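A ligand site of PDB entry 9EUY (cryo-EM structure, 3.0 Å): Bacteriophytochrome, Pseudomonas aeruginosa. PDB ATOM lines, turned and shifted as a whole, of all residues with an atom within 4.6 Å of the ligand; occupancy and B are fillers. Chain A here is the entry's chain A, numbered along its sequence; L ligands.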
ATOM      1  N   LEU A   9     -20.528   5.655  -0.991  1.00  0.00           N
ATOM      2  CA  LEU A   9     -21.206   4.975  -2.084  1.00  0.00           C
ATOM      3  C   LEU A   9     -22.372   4.099  -1.626  1.00  0.00           C
ATOM      4  O   LEU A   9     -23.257   3.799  -2.421  1.00  0.00           O
ATOM      5  CB  LEU A   9     -20.214   4.106  -2.859  1.00  0.00           C
ATOM      6  CG  LEU A   9     -19.209   4.781  -3.785  1.00  0.00           C
ATOM      7  CD1 LEU A   9     -18.166   3.787  -4.259  1.00  0.00           C
ATOM      8  CD2 LEU A   9     -19.942   5.374  -4.974  1.00  0.00           C
ATOM      9  N   CYS A  12     -25.029   7.254  -0.850  1.00  0.00           N
ATOM     10  CA  CYS A  12     -25.069   8.463  -1.664  1.00  0.00           C
ATOM     11  C   CYS A  12     -26.348   8.603  -2.489  1.00  0.00           C
ATOM     12  O   CYS A  12     -26.654   9.711  -2.930  1.00  0.00           O
ATOM     13  CB  CYS A  12     -23.861   8.495  -2.605  1.00  0.00           C
ATOM     14  SG  CYS A  12     -23.613  10.097  -3.404  1.00  0.00           S
ATOM     15  N   GLU A  13     -27.100   7.527  -2.696  1.00  0.00           N
ATOM     16  CA  GLU A  13     -28.360   7.652  -3.424  1.00  0.00           C
ATOM     17  C   GLU A  13     -29.440   8.345  -2.597  1.00  0.00           C
ATOM     18  O   GLU A  13     -30.411   8.842  -3.176  1.00  0.00           O
ATOM     19  CB  GLU A  13     -28.853   6.273  -3.849  1.00  0.00           C
ATOM     20  CG  GLU A  13     -27.940   5.578  -4.846  1.00  0.00           C
ATOM     21  CD  GLU A  13     -28.497   4.253  -5.325  1.00  0.00           C
ATOM     22  OE1 GLU A  13     -29.508   3.794  -4.765  1.00  0.00           O
ATOM     23  OE2 GLU A  13     -27.915   3.671  -6.271  1.00  0.00           O
ATOM     24  N   ILE A  17     -28.893  16.427  -0.901  1.00  0.00           N
ATOM     25  CA  ILE A  17     -28.069  17.484  -1.497  1.00  0.00           C
ATOM     26  C   ILE A  17     -28.772  18.831  -1.609  1.00  0.00           C
ATOM     27  O   ILE A  17     -28.111  19.833  -1.876  1.00  0.00           O
ATOM     28  CB  ILE A  17     -27.582  17.044  -2.892  1.00  0.00           C
ATOM     29  CG1 ILE A  17     -28.766  16.741  -3.808  1.00  0.00           C
ATOM     30  CG2 ILE A  17     -26.696  15.826  -2.768  1.00  0.00           C
ATOM     31  CD1 ILE A  17     -28.364  16.483  -5.235  1.00  0.00           C
ATOM     32  N   TYR A 163     -25.598  15.913 -23.120  1.00  0.00           N
ATOM     33  CA  TYR A 163     -26.107  14.631 -22.670  1.00  0.00           C
ATOM     34  C   TYR A 163     -27.549  14.481 -23.136  1.00  0.00           C
ATOM     35  O   TYR A 163     -28.303  15.449 -23.156  1.00  0.00           O
ATOM     36  CB  TYR A 163     -26.046  14.505 -21.154  1.00  0.00           C
ATOM     37  CG  TYR A 163     -24.692  14.721 -20.549  1.00  0.00           C
ATOM     38  CD1 TYR A 163     -23.645  13.851 -20.816  1.00  0.00           C
ATOM     39  CD2 TYR A 163     -24.455  15.769 -19.685  1.00  0.00           C
ATOM     40  CE1 TYR A 163     -22.405  14.040 -20.259  1.00  0.00           C
ATOM     41  CE2 TYR A 163     -23.231  15.964 -19.124  1.00  0.00           C
ATOM     42  CZ  TYR A 163     -22.206  15.099 -19.411  1.00  0.00           C
ATOM     43  OH  TYR A 163     -20.969  15.305 -18.837  1.00  0.00           O
ATOM     44  N   TYR A 185     -14.952  11.959 -24.917  1.00  0.00           N
ATOM     45  CA  TYR A 185     -15.960  11.143 -24.248  1.00  0.00           C
ATOM     46  C   TYR A 185     -17.189  10.901 -25.127  1.00  0.00           C
ATOM     47  O   TYR A 185     -18.186  10.366 -24.635  1.00  0.00           O
ATOM     48  CB  TYR A 185     -16.385  11.773 -22.929  1.00  0.00           C
ATOM     49  CG  TYR A 185     -15.274  11.846 -21.901  1.00  0.00           C
ATOM     50  CD1 TYR A 185     -14.492  10.735 -21.630  1.00  0.00           C
ATOM     51  CD2 TYR A 185     -15.016  13.024 -21.226  1.00  0.00           C
ATOM     52  CE1 TYR A 185     -13.477  10.795 -20.701  1.00  0.00           C
ATOM     53  CE2 TYR A 185     -13.997  13.091 -20.286  1.00  0.00           C
ATOM     54  CZ  TYR A 185     -13.232  11.977 -20.031  1.00  0.00           C
ATOM     55  OH  TYR A 185     -12.218  12.038 -19.102  1.00  0.00           O
ATOM     56  N   GLN A 188     -19.959   8.015 -24.810  1.00  0.00           N
ATOM     57  CA  GLN A 188     -19.941   7.387 -23.491  1.00  0.00           C
ATOM     58  C   GLN A 188     -21.345   7.251 -22.929  1.00  0.00           C
ATOM     59  O   GLN A 188     -22.202   8.123 -23.110  1.00  0.00           O
ATOM     60  CB  GLN A 188     -19.075   8.185 -22.522  1.00  0.00           C
ATOM     61  CG  GLN A 188     -19.163   7.686 -21.092  1.00  0.00           C
ATOM     62  CD  GLN A 188     -17.911   7.908 -20.298  1.00  0.00           C
ATOM     63  OE1 GLN A 188     -16.947   8.496 -20.791  1.00  0.00           O
ATOM     64  NE2 GLN A 188     -17.894   7.422 -19.070  1.00  0.00           N
ATOM     65  N   TYR A 190     -23.561   6.124 -19.236  1.00  0.00           N
ATOM     66  CA  TYR A 190     -23.439   5.967 -17.789  1.00  0.00           C
ATOM     67  C   TYR A 190     -24.804   5.704 -17.179  1.00  0.00           C
ATOM     68  O   TYR A 190     -25.824   6.114 -17.739  1.00  0.00           O
ATOM     69  CB  TYR A 190     -22.782   7.212 -17.150  1.00  0.00           C
ATOM     70  CG  TYR A 190     -23.415   8.531 -17.501  1.00  0.00           C
ATOM     71  CD1 TYR A 190     -24.564   8.974 -16.850  1.00  0.00           C
ATOM     72  CD2 TYR A 190     -22.853   9.349 -18.466  1.00  0.00           C
ATOM     73  CE1 TYR A 190     -25.117  10.190 -17.142  1.00  0.00           C
ATOM     74  CE2 TYR A 190     -23.415  10.567 -18.772  1.00  0.00           C
ATOM     75  CZ  TYR A 190     -24.543  10.989 -18.109  1.00  0.00           C
ATOM     76  OH  TYR A 190     -25.115  12.194 -18.439  1.00  0.00           O
ATOM     77  N   SER A 193     -27.893   5.886 -11.848  1.00  0.00           N
ATOM     78  CA  SER A 193     -27.352   6.119 -10.510  1.00  0.00           C
ATOM     79  C   SER A 193     -26.265   7.176 -10.489  1.00  0.00           C
ATOM     80  O   SER A 193     -25.914   7.639  -9.392  1.00  0.00           O
ATOM     81  CB  SER A 193     -26.815   4.806  -9.947  1.00  0.00           C
ATOM     82  OG  SER A 193     -25.876   4.214 -10.823  1.00  0.00           O
ATOM     83  N   ASP A 194     -25.722   7.566 -11.643  1.00  0.00           N
ATOM     84  CA  ASP A 194     -24.733   8.635 -11.682  1.00  0.00           C
ATOM     85  C   ASP A 194     -25.347  10.001 -11.408  1.00  0.00           C
ATOM     86  O   ASP A 194     -24.614  10.942 -11.097  1.00  0.00           O
ATOM     87  CB  ASP A 194     -24.027   8.635 -13.032  1.00  0.00           C
ATOM     88  CG  ASP A 194     -22.748   7.835 -13.031  1.00  0.00           C
ATOM     89  OD1 ASP A 194     -22.695   6.810 -12.309  1.00  0.00           O
ATOM     90  OD2 ASP A 194     -21.789   8.220 -13.727  1.00  0.00           O
ATOM     91  N   ILE A 195     -26.659  10.121 -11.527  1.00  0.00           N
ATOM     92  CA  ILE A 195     -27.392  11.349 -11.218  1.00  0.00           C
ATOM     93  C   ILE A 195     -28.618  10.965 -10.415  1.00  0.00           C
ATOM     94  O   ILE A 195     -29.669  10.649 -10.998  1.00  0.00           O
ATOM     95  CB  ILE A 195     -27.772  12.131 -12.493  1.00  0.00           C
ATOM     96  CG1 ILE A 195     -26.559  12.341 -13.399  1.00  0.00           C
ATOM     97  CG2 ILE A 195     -28.360  13.472 -12.128  1.00  0.00           C
ATOM     98  CD1 ILE A 195     -26.864  13.123 -14.647  1.00  0.00           C
ATOM     99  N   PRO A 196     -28.547  10.966  -9.080  1.00  0.00           N
ATOM    100  CA  PRO A 196     -29.671  10.522  -8.262  1.00  0.00           C
ATOM    101  C   PRO A 196     -30.917  11.374  -8.455  1.00  0.00           C
ATOM    102  O   PRO A 196     -30.866  12.516  -8.931  1.00  0.00           O
ATOM    103  CB  PRO A 196     -29.141  10.631  -6.830  1.00  0.00           C
ATOM    104  CG  PRO A 196     -28.098  11.688  -6.911  1.00  0.00           C
ATOM    105  CD  PRO A 196     -27.452  11.506  -8.261  1.00  0.00           C
ATOM    106  N   ALA A 199     -30.703  14.937  -7.603  1.00  0.00           N
ATOM    107  CA  ALA A 199     -29.946  15.755  -8.539  1.00  0.00           C
ATOM    108  C   ALA A 199     -30.755  16.004  -9.802  1.00  0.00           C
ATOM    109  O   ALA A 199     -30.721  17.109 -10.354  1.00  0.00           O
ATOM    110  CB  ALA A 199     -28.610  15.088  -8.864  1.00  0.00           C
ATOM    111  N   TYR A 203     -31.863  19.604 -11.299  1.00  0.00           N
ATOM    112  CA  TYR A 203     -31.619  20.005 -12.696  1.00  0.00           C
ATOM    113  C   TYR A 203     -32.908  20.362 -13.423  1.00  0.00           C
ATOM    114  O   TYR A 203     -32.879  21.117 -14.390  1.00  0.00           O
ATOM    115  CB  TYR A 203     -30.878  18.903 -13.447  1.00  0.00           C
ATOM    116  CG  TYR A 203     -29.406  18.833 -13.147  1.00  0.00           C
ATOM    117  CD1 TYR A 203     -28.591  19.943 -13.290  1.00  0.00           C
ATOM    118  CD2 TYR A 203     -28.811  17.649 -12.726  1.00  0.00           C
ATOM    119  CE1 TYR A 203     -27.240  19.878 -13.036  1.00  0.00           C
ATOM    120  CE2 TYR A 203     -27.462  17.580 -12.450  1.00  0.00           C
ATOM    121  CZ  TYR A 203     -26.682  18.698 -12.619  1.00  0.00           C
ATOM    122  OH  TYR A 203     -25.333  18.637 -12.323  1.00  0.00           O
ATOM    123  N   ARG A 209     -26.766  25.461 -13.367  1.00  0.00           N
ATOM    124  CA  ARG A 209     -25.975  24.979 -12.241  1.00  0.00           C
ATOM    125  C   ARG A 209     -24.518  25.292 -12.545  1.00  0.00           C
ATOM    126  O   ARG A 209     -24.024  24.960 -13.622  1.00  0.00           O
ATOM    127  CB  ARG A 209     -26.177  23.474 -12.048  1.00  0.00           C
ATOM    128  CG  ARG A 209     -25.325  22.829 -10.968  1.00  0.00           C
ATOM    129  CD  ARG A 209     -25.564  23.448  -9.609  1.00  0.00           C
ATOM    130  NE  ARG A 209     -24.907  22.700  -8.551  1.00  0.00           N
ATOM    131  CZ  ARG A 209     -24.690  23.154  -7.329  1.00  0.00           C
ATOM    132  NH1 ARG A 209     -24.931  24.413  -7.015  1.00  0.00           N
ATOM    133  NH2 ARG A 209     -24.183  22.340  -6.412  1.00  0.00           N
ATOM    134  N   ILE A 211     -20.406  25.302 -10.943  1.00  0.00           N
ATOM    135  CA  ILE A 211     -19.424  24.849  -9.967  1.00  0.00           C
ATOM    136  C   ILE A 211     -18.131  25.590 -10.289  1.00  0.00           C
ATOM    137  O   ILE A 211     -17.388  25.205 -11.200  1.00  0.00           O
ATOM    138  CB  ILE A 211     -19.212  23.333 -10.008  1.00  0.00           C
ATOM    139  CG1 ILE A 211     -20.535  22.614  -9.712  1.00  0.00           C
ATOM    140  CG2 ILE A 211     -18.150  22.915  -9.009  1.00  0.00           C
ATOM    141  CD1 ILE A 211     -20.475  21.128  -9.923  1.00  0.00           C
ATOM    142  N   ARG A 241     -25.415  26.967  -3.821  1.00  0.00           N
ATOM    143  CA  ARG A 241     -25.577  25.694  -3.135  1.00  0.00           C
ATOM    144  C   ARG A 241     -24.346  24.803  -3.288  1.00  0.00           C
ATOM    145  O   ARG A 241     -23.776  24.691  -4.375  1.00  0.00           O
ATOM    146  CB  ARG A 241     -26.824  24.969  -3.643  1.00  0.00           C
ATOM    147  CG  ARG A 241     -27.278  23.828  -2.776  1.00  0.00           C
ATOM    148  CD  ARG A 241     -28.463  23.106  -3.391  1.00  0.00           C
ATOM    149  NE  ARG A 241     -28.077  22.178  -4.445  1.00  0.00           N
ATOM    150  CZ  ARG A 241     -28.339  22.359  -5.731  1.00  0.00           C
ATOM    151  NH1 ARG A 241     -28.998  23.413  -6.164  1.00  0.00           N
ATOM    152  NH2 ARG A 241     -27.937  21.444  -6.609  1.00  0.00           N
ATOM    153  N   SER A 242     -23.934  24.202  -2.173  1.00  0.00           N
ATOM    154  CA  SER A 242     -22.797  23.285  -2.139  1.00  0.00           C
ATOM    155  C   SER A 242     -22.956  22.110  -3.103  1.00  0.00           C
ATOM    156  O   SER A 242     -24.048  21.791  -3.571  1.00  0.00           O
ATOM    157  CB  SER A 242     -22.584  22.765  -0.723  1.00  0.00           C
ATOM    158  OG  SER A 242     -21.300  22.195  -0.577  1.00  0.00           O
ATOM    159  N   VAL A 243     -21.822  21.471  -3.400  1.00  0.00           N
ATOM    160  CA  VAL A 243     -21.743  20.322  -4.291  1.00  0.00           C
ATOM    161  C   VAL A 243     -21.488  19.078  -3.445  1.00  0.00           C
ATOM    162  O   VAL A 243     -20.705  19.115  -2.490  1.00  0.00           O
ATOM    163  CB  VAL A 243     -20.626  20.502  -5.347  1.00  0.00           C
ATOM    164  CG1 VAL A 243     -20.759  19.459  -6.433  1.00  0.00           C
ATOM    165  CG2 VAL A 243     -20.673  21.898  -5.926  1.00  0.00           C
ATOM    166  N   SER A 244     -22.172  17.986  -3.786  1.00  0.00           N
ATOM    167  CA  SER A 244     -21.964  16.726  -3.084  1.00  0.00           C
ATOM    168  C   SER A 244     -20.480  16.354  -3.051  1.00  0.00           C
ATOM    169  O   SER A 244     -19.763  16.589  -4.027  1.00  0.00           O
ATOM    170  CB  SER A 244     -22.773  15.616  -3.761  1.00  0.00           C
ATOM    171  OG  SER A 244     -22.471  14.355  -3.186  1.00  0.00           O
ATOM    172  N   ILE A 246     -19.195  13.449  -3.343  1.00  0.00           N
ATOM    173  CA  ILE A 246     -18.923  12.391  -4.308  1.00  0.00           C
ATOM    174  C   ILE A 246     -18.830  12.920  -5.731  1.00  0.00           C
ATOM    175  O   ILE A 246     -17.998  12.448  -6.516  1.00  0.00           O
ATOM    176  CB  ILE A 246     -19.971  11.273  -4.163  1.00  0.00           C
ATOM    177  CG1 ILE A 246     -19.419  10.203  -3.206  1.00  0.00           C
ATOM    178  CG2 ILE A 246     -20.349  10.684  -5.508  1.00  0.00           C
ATOM    179  CD1 ILE A 246     -20.368   9.095  -2.874  1.00  0.00           C
ATOM    180  N   HIS A 247     -19.645  13.908  -6.101  1.00  0.00           N
ATOM    181  CA  HIS A 247     -19.446  14.513  -7.422  1.00  0.00           C
ATOM    182  C   HIS A 247     -18.179  15.368  -7.493  1.00  0.00           C
ATOM    183  O   HIS A 247     -17.543  15.430  -8.544  1.00  0.00           O
ATOM    184  CB  HIS A 247     -20.652  15.363  -7.805  1.00  0.00           C
ATOM    185  CG  HIS A 247     -20.724  15.666  -9.270  1.00  0.00           C
ATOM    186  ND1 HIS A 247     -20.734  14.682 -10.234  1.00  0.00           N
ATOM    187  CD2 HIS A 247     -20.772  16.841  -9.941  1.00  0.00           C
ATOM    188  CE1 HIS A 247     -20.796  15.228 -11.426  1.00  0.00           C
ATOM    189  NE2 HIS A 247     -20.823  16.544 -11.280  1.00  0.00           N
ATOM    190  N   TYR A 250     -15.649  12.677  -8.107  1.00  0.00           N
ATOM    191  CA  TYR A 250     -15.774  12.244  -9.493  1.00  0.00           C
ATOM    192  C   TYR A 250     -15.086  13.225 -10.440  1.00  0.00           C
ATOM    193  O   TYR A 250     -14.234  12.827 -11.242  1.00  0.00           O
ATOM    194  CB  TYR A 250     -17.254  12.090  -9.854  1.00  0.00           C
ATOM    195  CG  TYR A 250     -17.512  11.242 -11.075  1.00  0.00           C
ATOM    196  CD1 TYR A 250     -17.016  11.589 -12.315  1.00  0.00           C
ATOM    197  CD2 TYR A 250     -18.294  10.097 -10.977  1.00  0.00           C
ATOM    198  CE1 TYR A 250     -17.286  10.811 -13.423  1.00  0.00           C
ATOM    199  CE2 TYR A 250     -18.559   9.325 -12.074  1.00  0.00           C
ATOM    200  CZ  TYR A 250     -18.049   9.684 -13.301  1.00  0.00           C
ATOM    201  OH  TYR A 250     -18.302   8.886 -14.388  1.00  0.00           O
ATOM    202  N   MET A 254     -11.696  13.032 -12.996  1.00  0.00           N
ATOM    203  CA  MET A 254     -11.672  13.443 -14.390  1.00  0.00           C
ATOM    204  C   MET A 254     -10.675  14.553 -14.683  1.00  0.00           C
ATOM    205  O   MET A 254     -10.453  14.871 -15.857  1.00  0.00           O
ATOM    206  CB  MET A 254     -13.068  13.895 -14.838  1.00  0.00           C
ATOM    207  CG  MET A 254     -14.100  12.797 -14.886  1.00  0.00           C
ATOM    208  SD  MET A 254     -15.710  13.439 -15.393  1.00  0.00           S
ATOM    209  CE  MET A 254     -15.396  13.753 -17.127  1.00  0.00           C
ATOM    210  N   SER A 259     -17.335  23.476 -13.565  1.00  0.00           N
ATOM    211  CA  SER A 259     -18.406  22.965 -14.402  1.00  0.00           C
ATOM    212  C   SER A 259     -19.554  23.959 -14.432  1.00  0.00           C
ATOM    213  O   SER A 259     -19.821  24.660 -13.456  1.00  0.00           O
ATOM    214  CB  SER A 259     -18.900  21.607 -13.890  1.00  0.00           C
ATOM    215  OG  SER A 259     -20.043  21.185 -14.607  1.00  0.00           O
ATOM    216  N   LEU A 273     -29.032  17.676 -21.314  1.00  0.00           N
ATOM    217  CA  LEU A 273     -28.265  18.615 -20.504  1.00  0.00           C
ATOM    218  C   LEU A 273     -26.955  18.956 -21.213  1.00  0.00           C
ATOM    219  O   LEU A 273     -26.177  18.056 -21.521  1.00  0.00           O
ATOM    220  CB  LEU A 273     -27.986  18.004 -19.134  1.00  0.00           C
ATOM    221  CG  LEU A 273     -27.137  18.752 -18.119  1.00  0.00           C
ATOM    222  CD1 LEU A 273     -27.908  19.913 -17.520  1.00  0.00           C
ATOM    223  CD2 LEU A 273     -26.686  17.810 -17.026  1.00  0.00           C
ATOM    224  N   SER A 275     -23.377  20.237 -20.717  1.00  0.00           N
ATOM    225  CA  SER A 275     -22.467  20.408 -19.598  1.00  0.00           C
ATOM    226  C   SER A 275     -21.108  20.836 -20.100  1.00  0.00           C
ATOM    227  O   SER A 275     -20.522  20.191 -20.967  1.00  0.00           O
ATOM    228  CB  SER A 275     -22.333  19.118 -18.778  1.00  0.00           C
ATOM    229  OG  SER A 275     -21.582  19.335 -17.608  1.00  0.00           O
ATOM    230  N   HIS A 277     -17.220  21.628 -19.110  1.00  0.00           N
ATOM    231  CA  HIS A 277     -16.207  21.298 -18.123  1.00  0.00           C
ATOM    232  C   HIS A 277     -14.930  22.060 -18.433  1.00  0.00           C
ATOM    233  O   HIS A 277     -14.586  22.251 -19.605  1.00  0.00           O
ATOM    234  CB  HIS A 277     -15.905  19.796 -18.089  1.00  0.00           C
ATOM    235  CG  HIS A 277     -17.033  18.964 -17.560  1.00  0.00           C
ATOM    236  ND1 HIS A 277     -17.033  17.592 -17.662  1.00  0.00           N
ATOM    237  CD2 HIS A 277     -18.166  19.299 -16.905  1.00  0.00           C
ATOM    238  CE1 HIS A 277     -18.135  17.110 -17.109  1.00  0.00           C
ATOM    239  NE2 HIS A 277     -18.834  18.129 -16.642  1.00  0.00           N
ATOM    240  N   ARG A 453     -15.348   3.284  -9.200  1.00  0.00           N
ATOM    241  CA  ARG A 453     -16.634   3.681  -9.760  1.00  0.00           C
ATOM    242  C   ARG A 453     -16.761   5.191  -9.978  1.00  0.00           C
ATOM    243  O   ARG A 453     -17.531   5.615 -10.837  1.00  0.00           O
ATOM    244  CB  ARG A 453     -17.805   3.194  -8.897  1.00  0.00           C
ATOM    245  CG  ARG A 453     -19.130   3.538  -9.548  1.00  0.00           C
ATOM    246  CD  ARG A 453     -20.322   2.753  -9.061  1.00  0.00           C
ATOM    247  NE  ARG A 453     -21.656   3.139  -9.550  1.00  0.00           N
ATOM    248  CZ  ARG A 453     -21.978   4.043 -10.469  1.00  0.00           C
ATOM    249  NH1 ARG A 453     -21.086   4.693 -11.183  1.00  0.00           N
ATOM    250  NH2 ARG A 453     -23.271   4.300 -10.692  1.00  0.00           N
ATOM    251  N   LEU A 454     -15.989   6.004  -9.263  1.00  0.00           N
ATOM    252  CA  LEU A 454     -16.002   7.445  -9.535  1.00  0.00           C
ATOM    253  C   LEU A 454     -14.996   7.828 -10.624  1.00  0.00           C
ATOM    254  O   LEU A 454     -14.154   8.704 -10.446  1.00  0.00           O
ATOM    255  CB  LEU A 454     -15.769   8.231  -8.258  1.00  0.00           C
ATOM    256  CG  LEU A 454     -16.760   7.912  -7.142  1.00  0.00           C
ATOM    257  CD1 LEU A 454     -16.584   8.899  -6.008  1.00  0.00           C
ATOM    258  CD2 LEU A 454     -18.178   7.966  -7.657  1.00  0.00           C
ATOM    259  N   PRO A 456     -15.071   7.873 -15.300  1.00  0.00           N
ATOM    260  CA  PRO A 456     -15.846   7.557 -16.516  1.00  0.00           C
ATOM    261  C   PRO A 456     -15.915   6.079 -16.884  1.00  0.00           C
ATOM    262  O   PRO A 456     -16.992   5.578 -17.228  1.00  0.00           O
ATOM    263  CB  PRO A 456     -15.132   8.373 -17.597  1.00  0.00           C
ATOM    264  CG  PRO A 456     -14.576   9.543 -16.863  1.00  0.00           C
ATOM    265  CD  PRO A 456     -14.147   8.995 -15.524  1.00  0.00           C
ATOM    266  N   SER A 459     -18.207   4.284 -14.421  1.00  0.00           N
ATOM    267  CA  SER A 459     -19.595   4.521 -14.827  1.00  0.00           C
ATOM    268  C   SER A 459     -19.997   3.717 -16.056  1.00  0.00           C
ATOM    269  O   SER A 459     -21.121   3.210 -16.124  1.00  0.00           O
ATOM    270  CB  SER A 459     -19.795   6.014 -15.092  1.00  0.00           C
ATOM    271  OG  SER A 459     -19.671   6.761 -13.902  1.00  0.00           O
HETATM  272  C1  LIG L   1     -21.925   9.162  -8.916  1.00  0.00           C
HETATM  273  C2  LIG L   1     -24.172  12.935  -8.313  1.00  0.00           C
HETATM  274  O1  LIG L   1     -24.208  19.006  -6.920  1.00  0.00           O
HETATM  275  C3  LIG L   1     -23.702  14.192 -12.483  1.00  0.00           C
HETATM  276  O2  LIG L   1     -21.782  17.897 -15.479  1.00  0.00           O
HETATM  277  C4  LIG L   1     -21.049  11.270 -15.141  1.00  0.00           C
HETATM  278  C5  LIG L   1     -22.749   8.288  -8.007  1.00  0.00           C
HETATM  279  C6  LIG L   1     -24.588  14.202  -7.806  1.00  0.00           C
HETATM  280  O3  LIG L   1     -24.240  19.733  -9.019  1.00  0.00           O
HETATM  281  C7  LIG L   1     -23.884  14.651 -13.790  1.00  0.00           C
HETATM  282  O4  LIG L   1     -22.150  17.107 -13.431  1.00  0.00           O
HETATM  283  C8  LIG L   1     -20.119  12.169 -15.832  1.00  0.00           C
HETATM  284  C9  LIG L   1     -23.704   9.256  -7.366  1.00  0.00           C
HETATM  285  C10 LIG L   1     -24.624  15.084  -8.853  1.00  0.00           C
HETATM  286  C11 LIG L   1     -23.284  13.713 -14.643  1.00  0.00           C
HETATM  287  C12 LIG L   1     -19.386  11.441 -16.706  1.00  0.00           C
HETATM  288  C13 LIG L   1     -23.496  10.563  -7.986  1.00  0.00           C
HETATM  289  C14 LIG L   1     -24.273  14.359 -10.043  1.00  0.00           C
HETATM  290  C15 LIG L   1     -22.746  12.697 -13.841  1.00  0.00           C
HETATM  291  C16 LIG L   1     -19.863  10.042 -16.656  1.00  0.00           C
HETATM  292  C17 LIG L   1     -24.738   8.982  -6.587  1.00  0.00           C
HETATM  293  C18 LIG L   1     -25.018  16.510  -8.777  1.00  0.00           C
HETATM  294  C19 LIG L   1     -24.615  15.905 -14.123  1.00  0.00           C
HETATM  295  C20 LIG L   1     -18.326  11.925 -17.555  1.00  0.00           C
HETATM  296  C21 LIG L   1     -25.213   7.635  -6.167  1.00  0.00           C
HETATM  297  C22 LIG L   1     -23.807  17.438  -8.666  1.00  0.00           C
HETATM  298  C23 LIG L   1     -23.867  16.844 -15.071  1.00  0.00           C
HETATM  299  C24 LIG L   1     -17.503  11.198 -18.321  1.00  0.00           C
HETATM  300  C25 LIG L   1     -24.122  18.852  -8.147  1.00  0.00           C
HETATM  301  C26 LIG L   1     -22.478  17.329 -14.609  1.00  0.00           C
HETATM  302  C27 LIG L   1     -23.996  11.747  -7.561  1.00  0.00           C
HETATM  303  C28 LIG L   1     -24.175  14.835 -11.324  1.00  0.00           C
HETATM  304  C29 LIG L   1     -22.027  11.528 -14.231  1.00  0.00           C
HETATM  305  C30 LIG L   1     -21.784   7.586  -7.047  1.00  0.00           C
HETATM  306  C31 LIG L   1     -24.878  14.471  -6.373  1.00  0.00           C
HETATM  307  C32 LIG L   1     -23.243  13.756 -16.139  1.00  0.00           C
HETATM  308  C33 LIG L   1     -19.949  13.626 -15.530  1.00  0.00           C
HETATM  309  N1  LIG L   1     -22.431  10.437  -8.844  1.00  0.00           N
HETATM  310  O5  LIG L   1     -20.994   8.843  -9.605  1.00  0.00           O
HETATM  311  N2  LIG L   1     -24.003  13.068  -9.637  1.00  0.00           N
HETATM  312  N3  LIG L   1     -23.000  12.998 -12.529  1.00  0.00           N
HETATM  313  N4  LIG L   1     -20.867  10.027 -15.718  1.00  0.00           N
HETATM  314  O6  LIG L   1     -19.488   9.078 -17.275  1.00  0.00           O
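The side-chain hydroxyl (OG) of Ser 275 is in hydrogen-bond range of a ring nitrogen (NE2) of His 277 (3.2 Å).
OD2 of Asp 194 lies within hydrogen-bond range of OG of Ser 459 (2.6 Å).
The side-chain carboxylate of Asp 194 lies within salt-bridge range of the guanidinium group of Arg 453 (2.9 Å).
The side-chain amide nitrogen (NE2) of Gln 188 lies within hydrogen-bond range of the backbone carbonyl oxygen (O) of Pro 456.
The side-chain hydroxyl of Tyr 250 is in hydrogen-bond range of the side-chain hydroxyl of Ser 459, 2.6 Å away.
The backbone NH (N) of Ile 246 sits close to the side-chain hydroxyl (OG) of Ser 244 (3.4 Å).
O of Leu 273 is in hydrogen-bond range of N of Tyr 163 (2.7 Å).
The backbone NH of Ile 211 sits at hydrogen-bond distance from the backbone carbonyl oxygen of Ser 259 (2.7 Å).
The side-chain hydroxyl of Ser 275 sits at hydrogen-bond distance from an oxygen (O2) of the ligand, at 2.6 Å.
A ring nitrogen (NE2) of His 247 is in hydrogen-bond range of an oxygen (O4) of the ligand (2.6 Å).
The backbone carbonyl oxygen (O) of Asp 194 lies within hydrogen-bond range of a nitrogen (N2) of the ligand (2.7 Å).
OD2 of Asp 194 lies within hydrogen-bond range of N4 of the ligand.
An oxygen (O6) of the ligand is in hydrogen-bond range of the side-chain amide nitrogen (NE2) of Gln 188.
The side-chain hydroxyl (OH) of Tyr 250 sits close to a nitrogen (N4) of the ligand (3.1 Å).
The guanidinium group (NE) of Arg 209 lies within salt-bridge range of an oxygen (O3) of the ligand, at 3.1 Å.
An oxygen (O2) of the ligand lies within hydrogen-bond range of a ring nitrogen (NE2) of His 277.
CD2 of Leu 9 touches C30 of the ligand (3.5 Å).
Cys 12 touches the ligand.
Glu 13 touches the ligand (CG to C21, 3.7 Å).
Tyr 163 touches the ligand.
Tyr 190 touches the ligand (OH to C32, 3.4 Å).
Ser 193 touches the ligand (O to C21, 3.3 Å).
Ile 195 touches the ligand.
Pro 196 touches the ligand.
Ala 199 touches the ligand.
Tyr 203 touches the ligand.
Val 243 touches the ligand.
Ser 244 touches the ligand.
CG2 of Ile 246 touches C30 of the ligand, at 3.7 Å.
Met 254 touches the ligand.
Ser 259 touches the ligand (OG to O2, 3.8 Å).
CD2 of Leu 273 touches C23 of the ligand (3.6 Å).
Leu 454 touches the ligand.
Pro 456 touches the ligand (CG to C24, 3.7 Å).
Ser 459 touches the ligand (CB to O6, 3.8 Å).
Hydrophobic or aromatic side chains within 4 Å of the ligand: Leu 9, Tyr 163, Tyr 190, Ile 195, Pro 196, Ala 199, Tyr 203, Val 243, Ile 246, His 247, Tyr 250, Met 254, Leu 273, Leu 454 and Pro 456.
The nearest printed residue that does not touch the ligand is Ile 211 (4.1 Å).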
